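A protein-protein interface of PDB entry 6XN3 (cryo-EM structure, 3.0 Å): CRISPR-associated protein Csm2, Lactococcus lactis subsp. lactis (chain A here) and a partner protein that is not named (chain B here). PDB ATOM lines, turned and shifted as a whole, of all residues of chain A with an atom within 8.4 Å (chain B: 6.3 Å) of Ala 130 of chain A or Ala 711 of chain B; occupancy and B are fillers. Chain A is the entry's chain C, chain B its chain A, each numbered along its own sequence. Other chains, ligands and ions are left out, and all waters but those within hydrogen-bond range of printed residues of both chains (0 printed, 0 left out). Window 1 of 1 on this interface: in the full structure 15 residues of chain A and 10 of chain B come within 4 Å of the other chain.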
ATOM      1  N   PHE A  15      36.960  25.517  25.078  1.00  0.00           N
ATOM      2  CA  PHE A  15      35.599  25.239  25.535  1.00  0.00           C
ATOM      3  C   PHE A  15      34.781  24.541  24.462  1.00  0.00           C
ATOM      4  O   PHE A  15      33.929  23.702  24.773  1.00  0.00           O
ATOM      5  CB  PHE A  15      34.910  26.524  26.008  1.00  0.00           C
ATOM      6  CG  PHE A  15      34.775  27.583  24.956  1.00  0.00           C
ATOM      7  CD1 PHE A  15      33.663  27.636  24.136  1.00  0.00           C
ATOM      8  CD2 PHE A  15      35.742  28.551  24.817  1.00  0.00           C
ATOM      9  CE1 PHE A  15      33.552  28.595  23.174  1.00  0.00           C
ATOM     10  CE2 PHE A  15      35.618  29.533  23.867  1.00  0.00           C
ATOM     11  CZ  PHE A  15      34.520  29.556  23.049  1.00  0.00           C
ATOM     12  N   GLY A  16      35.028  24.870  23.195  1.00  0.00           N
ATOM     13  CA  GLY A  16      34.429  24.102  22.123  1.00  0.00           C
ATOM     14  C   GLY A  16      34.952  22.684  22.104  1.00  0.00           C
ATOM     15  O   GLY A  16      34.191  21.730  21.946  1.00  0.00           O
ATOM     16  N   ASP A  17      36.256  22.529  22.332  1.00  0.00           N
ATOM     17  CA  ASP A  17      36.866  21.205  22.355  1.00  0.00           C
ATOM     18  C   ASP A  17      36.435  20.418  23.585  1.00  0.00           C
ATOM     19  O   ASP A  17      36.162  19.216  23.491  1.00  0.00           O
ATOM     20  CB  ASP A  17      38.384  21.341  22.304  1.00  0.00           C
ATOM     21  CG  ASP A  17      38.862  22.027  21.041  1.00  0.00           C
ATOM     22  OD1 ASP A  17      38.275  21.783  19.965  1.00  0.00           O
ATOM     23  OD2 ASP A  17      39.810  22.834  21.132  1.00  0.00           O
ATOM     24  N   ALA A  19      33.601  20.869  25.291  1.00  0.00           N
ATOM     25  CA  ALA A  19      32.188  20.542  25.149  1.00  0.00           C
ATOM     26  C   ALA A  19      31.971  19.467  24.095  1.00  0.00           C
ATOM     27  O   ALA A  19      31.063  18.642  24.225  1.00  0.00           O
ATOM     28  CB  ALA A  19      31.389  21.797  24.812  1.00  0.00           C
ATOM     29  N   GLU A  20      32.798  19.457  23.048  1.00  0.00           N
ATOM     30  CA  GLU A  20      32.751  18.384  22.063  1.00  0.00           C
ATOM     31  C   GLU A  20      33.141  17.054  22.683  1.00  0.00           C
ATOM     32  O   GLU A  20      32.493  16.030  22.438  1.00  0.00           O
ATOM     33  CB  GLU A  20      33.676  18.710  20.898  1.00  0.00           C
ATOM     34  CG  GLU A  20      33.463  17.851  19.686  1.00  0.00           C
ATOM     35  CD  GLU A  20      34.528  18.083  18.650  1.00  0.00           C
ATOM     36  OE1 GLU A  20      35.714  18.155  19.033  1.00  0.00           O
ATOM     37  OE2 GLU A  20      34.184  18.191  17.457  1.00  0.00           O
ATOM     38  N   ILE A  23      30.148  16.018  25.051  1.00  0.00           N
ATOM     39  CA  ILE A  23      28.993  15.498  24.320  1.00  0.00           C
ATOM     40  C   ILE A  23      29.310  14.148  23.703  1.00  0.00           C
ATOM     41  O   ILE A  23      28.520  13.204  23.811  1.00  0.00           O
ATOM     42  CB  ILE A  23      28.528  16.510  23.258  1.00  0.00           C
ATOM     43  CG1 ILE A  23      27.846  17.695  23.920  1.00  0.00           C
ATOM     44  CG2 ILE A  23      27.567  15.876  22.262  1.00  0.00           C
ATOM     45  CD1 ILE A  23      26.599  17.308  24.668  1.00  0.00           C
ATOM     46  N   ILE A  46      17.536  20.557  27.294  1.00  0.00           N
ATOM     47  CA  ILE A  46      18.775  21.311  27.148  1.00  0.00           C
ATOM     48  C   ILE A  46      18.506  22.667  26.516  1.00  0.00           C
ATOM     49  O   ILE A  46      19.260  23.618  26.743  1.00  0.00           O
ATOM     50  CB  ILE A  46      19.842  20.529  26.362  1.00  0.00           C
ATOM     51  CG1 ILE A  46      19.406  20.291  24.928  1.00  0.00           C
ATOM     52  CG2 ILE A  46      20.163  19.235  27.044  1.00  0.00           C
ATOM     53  CD1 ILE A  46      20.530  19.931  24.044  1.00  0.00           C
ATOM     54  N   ARG A  47      17.416  22.807  25.758  1.00  0.00           N
ATOM     55  CA  ARG A  47      17.031  24.142  25.325  1.00  0.00           C
ATOM     56  C   ARG A  47      16.487  24.949  26.489  1.00  0.00           C
ATOM     57  O   ARG A  47      16.597  26.175  26.499  1.00  0.00           O
ATOM     58  CB  ARG A  47      16.013  24.081  24.192  1.00  0.00           C
ATOM     59  CG  ARG A  47      16.537  23.506  22.894  1.00  0.00           C
ATOM     60  CD  ARG A  47      17.832  24.124  22.454  1.00  0.00           C
ATOM     61  NE  ARG A  47      17.737  25.568  22.372  1.00  0.00           N
ATOM     62  CZ  ARG A  47      18.107  26.266  21.312  1.00  0.00           C
ATOM     63  NH1 ARG A  47      18.566  25.643  20.243  1.00  0.00           N
ATOM     64  NH2 ARG A  47      17.995  27.584  21.315  1.00  0.00           N
ATOM     65  N   LEU A  50      19.734  26.152  28.035  1.00  0.00           N
ATOM     66  CA  LEU A  50      20.279  27.224  27.214  1.00  0.00           C
ATOM     67  C   LEU A  50      19.454  28.494  27.328  1.00  0.00           C
ATOM     68  O   LEU A  50      20.014  29.591  27.321  1.00  0.00           O
ATOM     69  CB  LEU A  50      20.368  26.773  25.759  1.00  0.00           C
ATOM     70  CG  LEU A  50      20.927  27.785  24.762  1.00  0.00           C
ATOM     71  CD1 LEU A  50      22.317  28.223  25.158  1.00  0.00           C
ATOM     72  CD2 LEU A  50      20.924  27.232  23.364  1.00  0.00           C
ATOM     73  N   ARG A 123      29.526  30.817  26.228  1.00  0.00           N
ATOM     74  CA  ARG A 123      29.972  30.203  24.983  1.00  0.00           C
ATOM     75  C   ARG A 123      30.231  28.715  25.172  1.00  0.00           C
ATOM     76  O   ARG A 123      30.076  27.931  24.229  1.00  0.00           O
ATOM     77  CB  ARG A 123      31.224  30.897  24.445  1.00  0.00           C
ATOM     78  CG  ARG A 123      31.173  32.402  24.383  1.00  0.00           C
ATOM     79  CD  ARG A 123      30.929  33.018  23.039  1.00  0.00           C
ATOM     80  NE  ARG A 123      30.923  34.477  23.137  1.00  0.00           N
ATOM     81  CZ  ARG A 123      32.006  35.246  23.247  1.00  0.00           C
ATOM     82  NH1 ARG A 123      33.222  34.717  23.246  1.00  0.00           N
ATOM     83  NH2 ARG A 123      31.870  36.559  23.337  1.00  0.00           N
ATOM     84  N   TYR A 124      30.595  28.300  26.392  1.00  0.00           N
ATOM     85  CA  TYR A 124      30.736  26.877  26.688  1.00  0.00           C
ATOM     86  C   TYR A 124      29.403  26.148  26.569  1.00  0.00           C
ATOM     87  O   TYR A 124      29.313  25.095  25.924  1.00  0.00           O
ATOM     88  CB  TYR A 124      31.325  26.711  28.087  1.00  0.00           C
ATOM     89  CG  TYR A 124      31.380  25.295  28.597  1.00  0.00           C
ATOM     90  CD1 TYR A 124      32.345  24.413  28.141  1.00  0.00           C
ATOM     91  CD2 TYR A 124      30.481  24.847  29.551  1.00  0.00           C
ATOM     92  CE1 TYR A 124      32.406  23.125  28.614  1.00  0.00           C
ATOM     93  CE2 TYR A 124      30.533  23.563  30.029  1.00  0.00           C
ATOM     94  CZ  TYR A 124      31.497  22.708  29.558  1.00  0.00           C
ATOM     95  OH  TYR A 124      31.548  21.423  30.036  1.00  0.00           O
ATOM     96  N   VAL A 125      28.347  26.714  27.157  1.00  0.00           N
ATOM     97  CA  VAL A 125      27.030  26.086  27.083  1.00  0.00           C
ATOM     98  C   VAL A 125      26.477  26.151  25.663  1.00  0.00           C
ATOM     99  O   VAL A 125      25.836  25.205  25.190  1.00  0.00           O
ATOM    100  CB  VAL A 125      26.079  26.729  28.105  1.00  0.00           C
ATOM    101  CG1 VAL A 125      24.708  26.085  28.066  1.00  0.00           C
ATOM    102  CG2 VAL A 125      26.650  26.583  29.481  1.00  0.00           C
ATOM    103  N   GLU A 126      26.739  27.253  24.955  1.00  0.00           N
ATOM    104  CA  GLU A 126      26.310  27.385  23.564  1.00  0.00           C
ATOM    105  C   GLU A 126      26.968  26.337  22.675  1.00  0.00           C
ATOM    106  O   GLU A 126      26.300  25.708  21.846  1.00  0.00           O
ATOM    107  CB  GLU A 126      26.631  28.793  23.069  1.00  0.00           C
ATOM    108  CG  GLU A 126      26.424  29.017  21.587  1.00  0.00           C
ATOM    109  CD  GLU A 126      26.832  30.412  21.140  1.00  0.00           C
ATOM    110  OE1 GLU A 126      26.572  31.375  21.887  1.00  0.00           O
ATOM    111  OE2 GLU A 126      27.393  30.550  20.033  1.00  0.00           O
ATOM    112  N   SER A 127      28.266  26.096  22.879  1.00  0.00           N
ATOM    113  CA  SER A 127      28.965  25.044  22.151  1.00  0.00           C
ATOM    114  C   SER A 127      28.454  23.668  22.540  1.00  0.00           C
ATOM    115  O   SER A 127      28.425  22.753  21.710  1.00  0.00           O
ATOM    116  CB  SER A 127      30.454  25.139  22.430  1.00  0.00           C
ATOM    117  OG  SER A 127      30.687  24.915  23.802  1.00  0.00           O
ATOM    118  N   LEU A 128      28.054  23.507  23.801  1.00  0.00           N
ATOM    119  CA  LEU A 128      27.525  22.233  24.281  1.00  0.00           C
ATOM    120  C   LEU A 128      26.209  21.890  23.586  1.00  0.00           C
ATOM    121  O   LEU A 128      26.013  20.763  23.107  1.00  0.00           O
ATOM    122  CB  LEU A 128      27.343  22.337  25.792  1.00  0.00           C
ATOM    123  CG  LEU A 128      26.888  21.214  26.704  1.00  0.00           C
ATOM    124  CD1 LEU A 128      27.908  20.122  26.650  1.00  0.00           C
ATOM    125  CD2 LEU A 128      26.750  21.734  28.113  1.00  0.00           C
ATOM    126  N   ILE A 129      25.318  22.882  23.480  1.00  0.00           N
ATOM    127  CA  ILE A 129      24.054  22.718  22.760  1.00  0.00           C
ATOM    128  C   ILE A 129      24.320  22.467  21.280  1.00  0.00           C
ATOM    129  O   ILE A 129      23.659  21.634  20.636  1.00  0.00           O
ATOM    130  CB  ILE A 129      23.164  23.960  22.953  1.00  0.00           C
ATOM    131  CG1 ILE A 129      22.872  24.210  24.426  1.00  0.00           C
ATOM    132  CG2 ILE A 129      21.849  23.809  22.218  1.00  0.00           C
ATOM    133  CD1 ILE A 129      22.156  23.121  25.095  1.00  0.00           C
ATOM    134  N   ALA A 130      25.305  23.187  20.730  1.00  0.00           N
ATOM    135  CA  ALA A 130      25.655  23.066  19.320  1.00  0.00           C
ATOM    136  C   ALA A 130      26.123  21.663  18.981  1.00  0.00           C
ATOM    137  O   ALA A 130      25.689  21.071  17.990  1.00  0.00           O
ATOM    138  CB  ALA A 130      26.746  24.071  18.980  1.00  0.00           C
ATOM    139  N   TYR A 131      26.979  21.098  19.825  1.00  0.00           N
ATOM    140  CA  TYR A 131      27.489  19.767  19.547  1.00  0.00           C
ATOM    141  C   TYR A 131      26.454  18.692  19.842  1.00  0.00           C
ATOM    142  O   TYR A 131      26.481  17.631  19.204  1.00  0.00           O
ATOM    143  CB  TYR A 131      28.776  19.555  20.327  1.00  0.00           C
ATOM    144  CG  TYR A 131      29.945  20.176  19.620  1.00  0.00           C
ATOM    145  CD1 TYR A 131      30.097  20.039  18.250  1.00  0.00           C
ATOM    146  CD2 TYR A 131      30.850  20.969  20.302  1.00  0.00           C
ATOM    147  CE1 TYR A 131      31.151  20.624  17.591  1.00  0.00           C
ATOM    148  CE2 TYR A 131      31.904  21.565  19.651  1.00  0.00           C
ATOM    149  CZ  TYR A 131      32.050  21.389  18.298  1.00  0.00           C
ATOM    150  OH  TYR A 131      33.109  21.983  17.655  1.00  0.00           O
ATOM    151  N   PHE A 132      25.525  18.949  20.774  1.00  0.00           N
ATOM    152  CA  PHE A 132      24.423  18.010  20.972  1.00  0.00           C
ATOM    153  C   PHE A 132      23.524  17.946  19.748  1.00  0.00           C
ATOM    154  O   PHE A 132      23.043  16.868  19.382  1.00  0.00           O
ATOM    155  CB  PHE A 132      23.595  18.376  22.198  1.00  0.00           C
ATOM    156  CG  PHE A 132      22.726  17.250  22.696  1.00  0.00           C
ATOM    157  CD1 PHE A 132      21.441  17.065  22.206  1.00  0.00           C
ATOM    158  CD2 PHE A 132      23.204  16.367  23.648  1.00  0.00           C
ATOM    159  CE1 PHE A 132      20.653  16.038  22.665  1.00  0.00           C
ATOM    160  CE2 PHE A 132      22.418  15.336  24.108  1.00  0.00           C
ATOM    161  CZ  PHE A 132      21.144  15.173  23.614  1.00  0.00           C
ATOM    162  N   LYS A 133      23.258  19.087  19.115  1.00  0.00           N
ATOM    163  CA  LYS A 133      22.484  19.021  17.882  1.00  0.00           C
ATOM    164  C   LYS A 133      23.315  18.454  16.736  1.00  0.00           C
ATOM    165  O   LYS A 133      22.771  17.788  15.848  1.00  0.00           O
ATOM    166  CB  LYS A 133      21.919  20.396  17.523  1.00  0.00           C
ATOM    167  CG  LYS A 133      20.914  20.338  16.382  1.00  0.00           C
ATOM    168  CD  LYS A 133      20.033  21.551  16.288  1.00  0.00           C
ATOM    169  CE  LYS A 133      19.208  21.477  15.021  1.00  0.00           C
ATOM    170  NZ  LYS A 133      18.411  20.219  14.979  1.00  0.00           N
ATOM    171  N   PHE A 134      24.632  18.680  16.757  1.00  0.00           N
ATOM    172  CA  PHE A 134      25.495  18.182  15.691  1.00  0.00           C
ATOM    173  C   PHE A 134      25.571  16.665  15.690  1.00  0.00           C
ATOM    174  O   PHE A 134      25.554  16.041  14.625  1.00  0.00           O
ATOM    175  CB  PHE A 134      26.891  18.781  15.822  1.00  0.00           C
ATOM    176  CG  PHE A 134      27.871  18.262  14.812  1.00  0.00           C
ATOM    177  CD1 PHE A 134      27.657  18.462  13.465  1.00  0.00           C
ATOM    178  CD2 PHE A 134      28.995  17.563  15.209  1.00  0.00           C
ATOM    179  CE1 PHE A 134      28.543  17.985  12.530  1.00  0.00           C
ATOM    180  CE2 PHE A 134      29.892  17.092  14.274  1.00  0.00           C
ATOM    181  CZ  PHE A 134      29.658  17.299  12.936  1.00  0.00           C
ATOM    182  N   TYR A 135      25.645  16.051  16.864  1.00  0.00           N
ATOM    183  CA  TYR A 135      25.746  14.601  16.952  1.00  0.00           C
ATOM    184  C   TYR A 135      24.366  13.988  17.164  1.00  0.00           C
ATOM    185  O   TYR A 135      23.725  14.232  18.190  1.00  0.00           O
ATOM    186  CB  TYR A 135      26.696  14.190  18.073  1.00  0.00           C
ATOM    187  CG  TYR A 135      28.152  14.423  17.751  1.00  0.00           C
ATOM    188  CD1 TYR A 135      28.681  14.039  16.529  1.00  0.00           C
ATOM    189  CD2 TYR A 135      29.005  15.001  18.680  1.00  0.00           C
ATOM    190  CE1 TYR A 135      30.012  14.238  16.235  1.00  0.00           C
ATOM    191  CE2 TYR A 135      30.341  15.203  18.392  1.00  0.00           C
ATOM    192  CZ  TYR A 135      30.836  14.822  17.170  1.00  0.00           C
ATOM    193  OH  TYR A 135      32.163  15.023  16.882  1.00  0.00           O
ATOM    194  N   GLY A 136      23.921  13.192  16.191  1.00  0.00           N
ATOM    195  CA  GLY A 136      22.717  12.386  16.298  1.00  0.00           C
ATOM    196  C   GLY A 136      21.419  13.147  16.450  1.00  0.00           C
ATOM    197  O   GLY A 136      20.582  12.781  17.280  1.00  0.00           O
ATOM    198  N   GLN B 706      38.005  31.229  17.581  1.00  0.00           N
ATOM    199  CA  GLN B 706      38.163  30.006  16.808  1.00  0.00           C
ATOM    200  C   GLN B 706      37.172  28.938  17.252  1.00  0.00           C
ATOM    201  O   GLN B 706      36.645  28.189  16.424  1.00  0.00           O
ATOM    202  CB  GLN B 706      39.612  29.529  16.914  1.00  0.00           C
ATOM    203  CG  GLN B 706      40.014  28.372  16.004  1.00  0.00           C
ATOM    204  CD  GLN B 706      39.729  27.013  16.574  1.00  0.00           C
ATOM    205  OE1 GLN B 706      39.735  26.827  17.786  1.00  0.00           O
ATOM    206  NE2 GLN B 706      39.500  26.046  15.703  1.00  0.00           N
ATOM    207  N   GLN B 707      36.900  28.853  18.551  1.00  0.00           N
ATOM    208  CA  GLN B 707      36.074  27.780  19.091  1.00  0.00           C
ATOM    209  C   GLN B 707      34.584  27.984  18.860  1.00  0.00           C
ATOM    210  O   GLN B 707      33.906  27.074  18.359  1.00  0.00           O
ATOM    211  CB  GLN B 707      36.338  27.635  20.589  1.00  0.00           C
ATOM    212  CG  GLN B 707      37.745  27.209  20.934  1.00  0.00           C
ATOM    213  CD  GLN B 707      38.008  25.770  20.561  1.00  0.00           C
ATOM    214  OE1 GLN B 707      37.570  24.858  21.251  1.00  0.00           O
ATOM    215  NE2 GLN B 707      38.711  25.557  19.465  1.00  0.00           N
ATOM    216  N   ILE B 708      34.058  29.162  19.208  1.00  0.00           N
ATOM    217  CA  ILE B 708      32.610  29.345  19.212  1.00  0.00           C
ATOM    218  C   ILE B 708      32.067  29.419  17.791  1.00  0.00           C
ATOM    219  O   ILE B 708      30.929  29.015  17.528  1.00  0.00           O
ATOM    220  CB  ILE B 708      32.218  30.572  20.061  1.00  0.00           C
ATOM    221  CG1 ILE B 708      30.722  30.541  20.369  1.00  0.00           C
ATOM    222  CG2 ILE B 708      32.631  31.881  19.411  1.00  0.00           C
ATOM    223  CD1 ILE B 708      30.296  29.326  21.157  1.00  0.00           C
ATOM    224  N   ASN B 709      32.884  29.867  16.842  1.00  0.00           N
ATOM    225  CA  ASN B 709      32.420  29.894  15.465  1.00  0.00           C
ATOM    226  C   ASN B 709      32.411  28.502  14.858  1.00  0.00           C
ATOM    227  O   ASN B 709      31.551  28.203  14.030  1.00  0.00           O
ATOM    228  CB  ASN B 709      33.277  30.845  14.652  1.00  0.00           C
ATOM    229  CG  ASN B 709      33.060  32.278  15.047  1.00  0.00           C
ATOM    230  OD1 ASN B 709      31.995  32.844  14.818  1.00  0.00           O
ATOM    231  ND2 ASN B 709      34.061  32.869  15.673  1.00  0.00           N
ATOM    232  N   ILE B 710      33.333  27.634  15.278  1.00  0.00           N
ATOM    233  CA  ILE B 710      33.290  26.237  14.856  1.00  0.00           C
ATOM    234  C   ILE B 710      32.056  25.549  15.428  1.00  0.00           C
ATOM    235  O   ILE B 710      31.378  24.775  14.733  1.00  0.00           O
ATOM    236  CB  ILE B 710      34.601  25.534  15.257  1.00  0.00           C
ATOM    237  CG1 ILE B 710      35.695  25.888  14.256  1.00  0.00           C
ATOM    238  CG2 ILE B 710      34.444  24.027  15.352  1.00  0.00           C
ATOM    239  CD1 ILE B 710      35.510  25.265  12.899  1.00  0.00           C
ATOM    240  N   ALA B 711      31.718  25.861  16.682  1.00  0.00           N
ATOM    241  CA  ALA B 711      30.500  25.319  17.284  1.00  0.00           C
ATOM    242  C   ALA B 711      29.245  25.812  16.570  1.00  0.00           C
ATOM    243  O   ALA B 711      28.343  25.016  16.273  1.00  0.00           O
ATOM    244  CB  ALA B 711      30.443  25.690  18.758  1.00  0.00           C
ATOM    245  N   ARG B 712      29.185  27.113  16.263  1.00  0.00           N
ATOM    246  CA  ARG B 712      28.045  27.669  15.534  1.00  0.00           C
ATOM    247  C   ARG B 712      27.962  27.099  14.130  1.00  0.00           C
ATOM    248  O   ARG B 712      26.867  26.908  13.590  1.00  0.00           O
ATOM    249  CB  ARG B 712      28.151  29.189  15.471  1.00  0.00           C
ATOM    250  CG  ARG B 712      27.803  29.890  16.757  1.00  0.00           C
ATOM    251  CD  ARG B 712      28.135  31.362  16.673  1.00  0.00           C
ATOM    252  NE  ARG B 712      28.163  31.984  17.988  1.00  0.00           N
ATOM    253  CZ  ARG B 712      28.719  33.160  18.237  1.00  0.00           C
ATOM    254  NH1 ARG B 712      29.289  33.839  17.253  1.00  0.00           N
ATOM    255  NH2 ARG B 712      28.705  33.658  19.463  1.00  0.00           N
ATOM    256  N   LEU B 713      29.115  26.806  13.537  1.00  0.00           N
ATOM    257  CA  LEU B 713      29.168  26.199  12.219  1.00  0.00           C
ATOM    258  C   LEU B 713      28.578  24.800  12.229  1.00  0.00           C
ATOM    259  O   LEU B 713      27.783  24.447  11.349  1.00  0.00           O
ATOM    260  CB  LEU B 713      30.615  26.172  11.761  1.00  0.00           C
ATOM    261  CG  LEU B 713      30.882  25.595  10.397  1.00  0.00           C
ATOM    262  CD1 LEU B 713      30.148  26.392   9.366  1.00  0.00           C
ATOM    263  CD2 LEU B 713      32.352  25.710  10.207  1.00  0.00           C
ATOM    264  N   ALA B 714      28.950  23.996  13.230  1.00  0.00           N
ATOM    265  CA  ALA B 714      28.386  22.654  13.359  1.00  0.00           C
ATOM    266  C   ALA B 714      26.889  22.710  13.618  1.00  0.00           C
ATOM    267  O   ALA B 714      26.121  21.919  13.051  1.00  0.00           O
ATOM    268  CB  ALA B 714      29.089  21.894  14.479  1.00  0.00           C
ATOM    269  N   TYR B 715      26.462  23.674  14.439  1.00  0.00           N
ATOM    270  CA  TYR B 715      25.046  23.847  14.746  1.00  0.00           C
ATOM    271  C   TYR B 715      24.244  24.217  13.506  1.00  0.00           C
ATOM    272  O   TYR B 715      23.172  23.656  13.267  1.00  0.00           O
ATOM    273  CB  TYR B 715      24.888  24.907  15.832  1.00  0.00           C
ATOM    274  CG  TYR B 715      23.465  25.280  16.137  1.00  0.00           C
ATOM    275  CD1 TYR B 715      22.645  24.430  16.856  1.00  0.00           C
ATOM    276  CD2 TYR B 715      22.940  26.487  15.705  1.00  0.00           C
ATOM    277  CE1 TYR B 715      21.345  24.773  17.139  1.00  0.00           C
ATOM    278  CE2 TYR B 715      21.642  26.836  15.983  1.00  0.00           C
ATOM    279  CZ  TYR B 715      20.849  25.971  16.695  1.00  0.00           C
ATOM    280  OH  TYR B 715      19.552  26.315  16.976  1.00  0.00           O
ATOM    281  N   THR B 716      24.766  25.127  12.681  1.00  0.00           N
ATOM    282  CA  THR B 716      24.040  25.527  11.478  1.00  0.00           C
ATOM    283  C   THR B 716      24.043  24.433  10.429  1.00  0.00           C
ATOM    284  O   THR B 716      23.066  24.280   9.684  1.00  0.00           O
ATOM    285  CB  THR B 716      24.639  26.789  10.882  1.00  0.00           C
ATOM    286  OG1 THR B 716      26.062  26.659  10.842  1.00  0.00           O
ATOM    287  CG2 THR B 716      24.255  27.973  11.705  1.00  0.00           C
ATOM    288  N   SER B 718      24.120  21.120  10.937  1.00  0.00           N
ATOM    289  CA  SER B 718      23.119  20.114  11.284  1.00  0.00           C
ATOM    290  C   SER B 718      21.712  20.693  11.316  1.00  0.00           C
ATOM    291  O   SER B 718      20.740  19.944  11.171  1.00  0.00           O
ATOM    292  CB  SER B 718      23.456  19.458  12.613  1.00  0.00           C
ATOM    293  OG  SER B 718      24.670  18.750  12.503  1.00  0.00           O
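The side-chain amide oxygen of Gln 707 of chain B is in hydrogen-bond range of the backbone NH of Gly 16 of chain A.
The side-chain amide oxygen of Gln 707 of chain B is in hydrogen-bond range of the backbone NH of Asp 17 of chain A.
NE of Arg 712 of chain B is in salt-bridge range of OE2 of Glu 126 of chain A, 2.6 Å away.
OH of Tyr 715 of chain B lies within hydrogen-bond range of NH1 of Arg 47 of chain A (3.5 Å).
The backbone carbonyl oxygen (O) of Arg 712 of chain B lies within hydrogen-bond range of the side-chain hydroxyl (OG1) of Thr 716 of chain B (2.9 Å).
The backbone carbonyl oxygen (O) of Arg 123 of chain A lies within hydrogen-bond range of the side-chain hydroxyl (OG) of Ser 127 of chain A (3.1 Å).
The side-chain hydroxyl (OG) of Ser 127 of chain A sits at hydrogen-bond distance from the backbone carbonyl oxygen (O) of Tyr 124 of chain A (2.5 Å).
Among the printed residues, pairs that only touch across the chains: Phe 134 of chain A with Ser 718 of chain B (3.2 Å), Ala 130 of chain A with Ala 711 of chain B (3.3 Å), Glu 126 of chain A with Ile 708 of chain B (3.3 Å), Tyr 131 of chain A with Ile 710 of chain B (3.4 Å), Arg 123 of chain A with Ile 708 of chain B (3.4 Å), Lys 133 of chain A with Tyr 715 of chain B (3.6 Å), Phe 15 of chain A with Gln 707 of chain B (3.6 Å), Lys 133 of chain A with Ser 718 of chain B (3.7 Å), Ser 127 of chain A with Ala 711 of chain B (3.7 Å), Ala 130 of chain A with Tyr 715 of chain B (3.7 Å), Phe 134 of chain A with Ala 714 of chain B (3.8 Å), Phe 15 of chain A with Ile 708 of chain B (3.9 Å) and Tyr 131 of chain A with Ala 714 of chain B (3.9 Å).
Of the printed residues of chain B, Phe 15 of chain A touches Gln 707 (3.6 Å) and Ile 708 (3.9 Å).
Printed residues of chain B within 4 Å of Arg 123 of chain A: Ile 708 (3.4 Å).
Printed residues of chain B within 4 Å of Glu 126 of chain A: Ile 708 (3.3 Å) and Arg 712 (2.6 Å).
Ala 130 of chain A touches two residues of chain B.
Of chain A, only Ser 127 (3.7 Å) and Ala 130 (3.3 Å) come within 4 Å of Ala 711 of chain B.
Of the printed residues of chain A, Arg 712 of chain B touches Glu 126.
Of the 12 printed residues of chain B, 8 touch a printed residue of chain A.
Along chain B the printed residues that touch a printed residue of chain A span positions 707 to 718.
Among the printed residues, 17 pairs touch across the chains.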
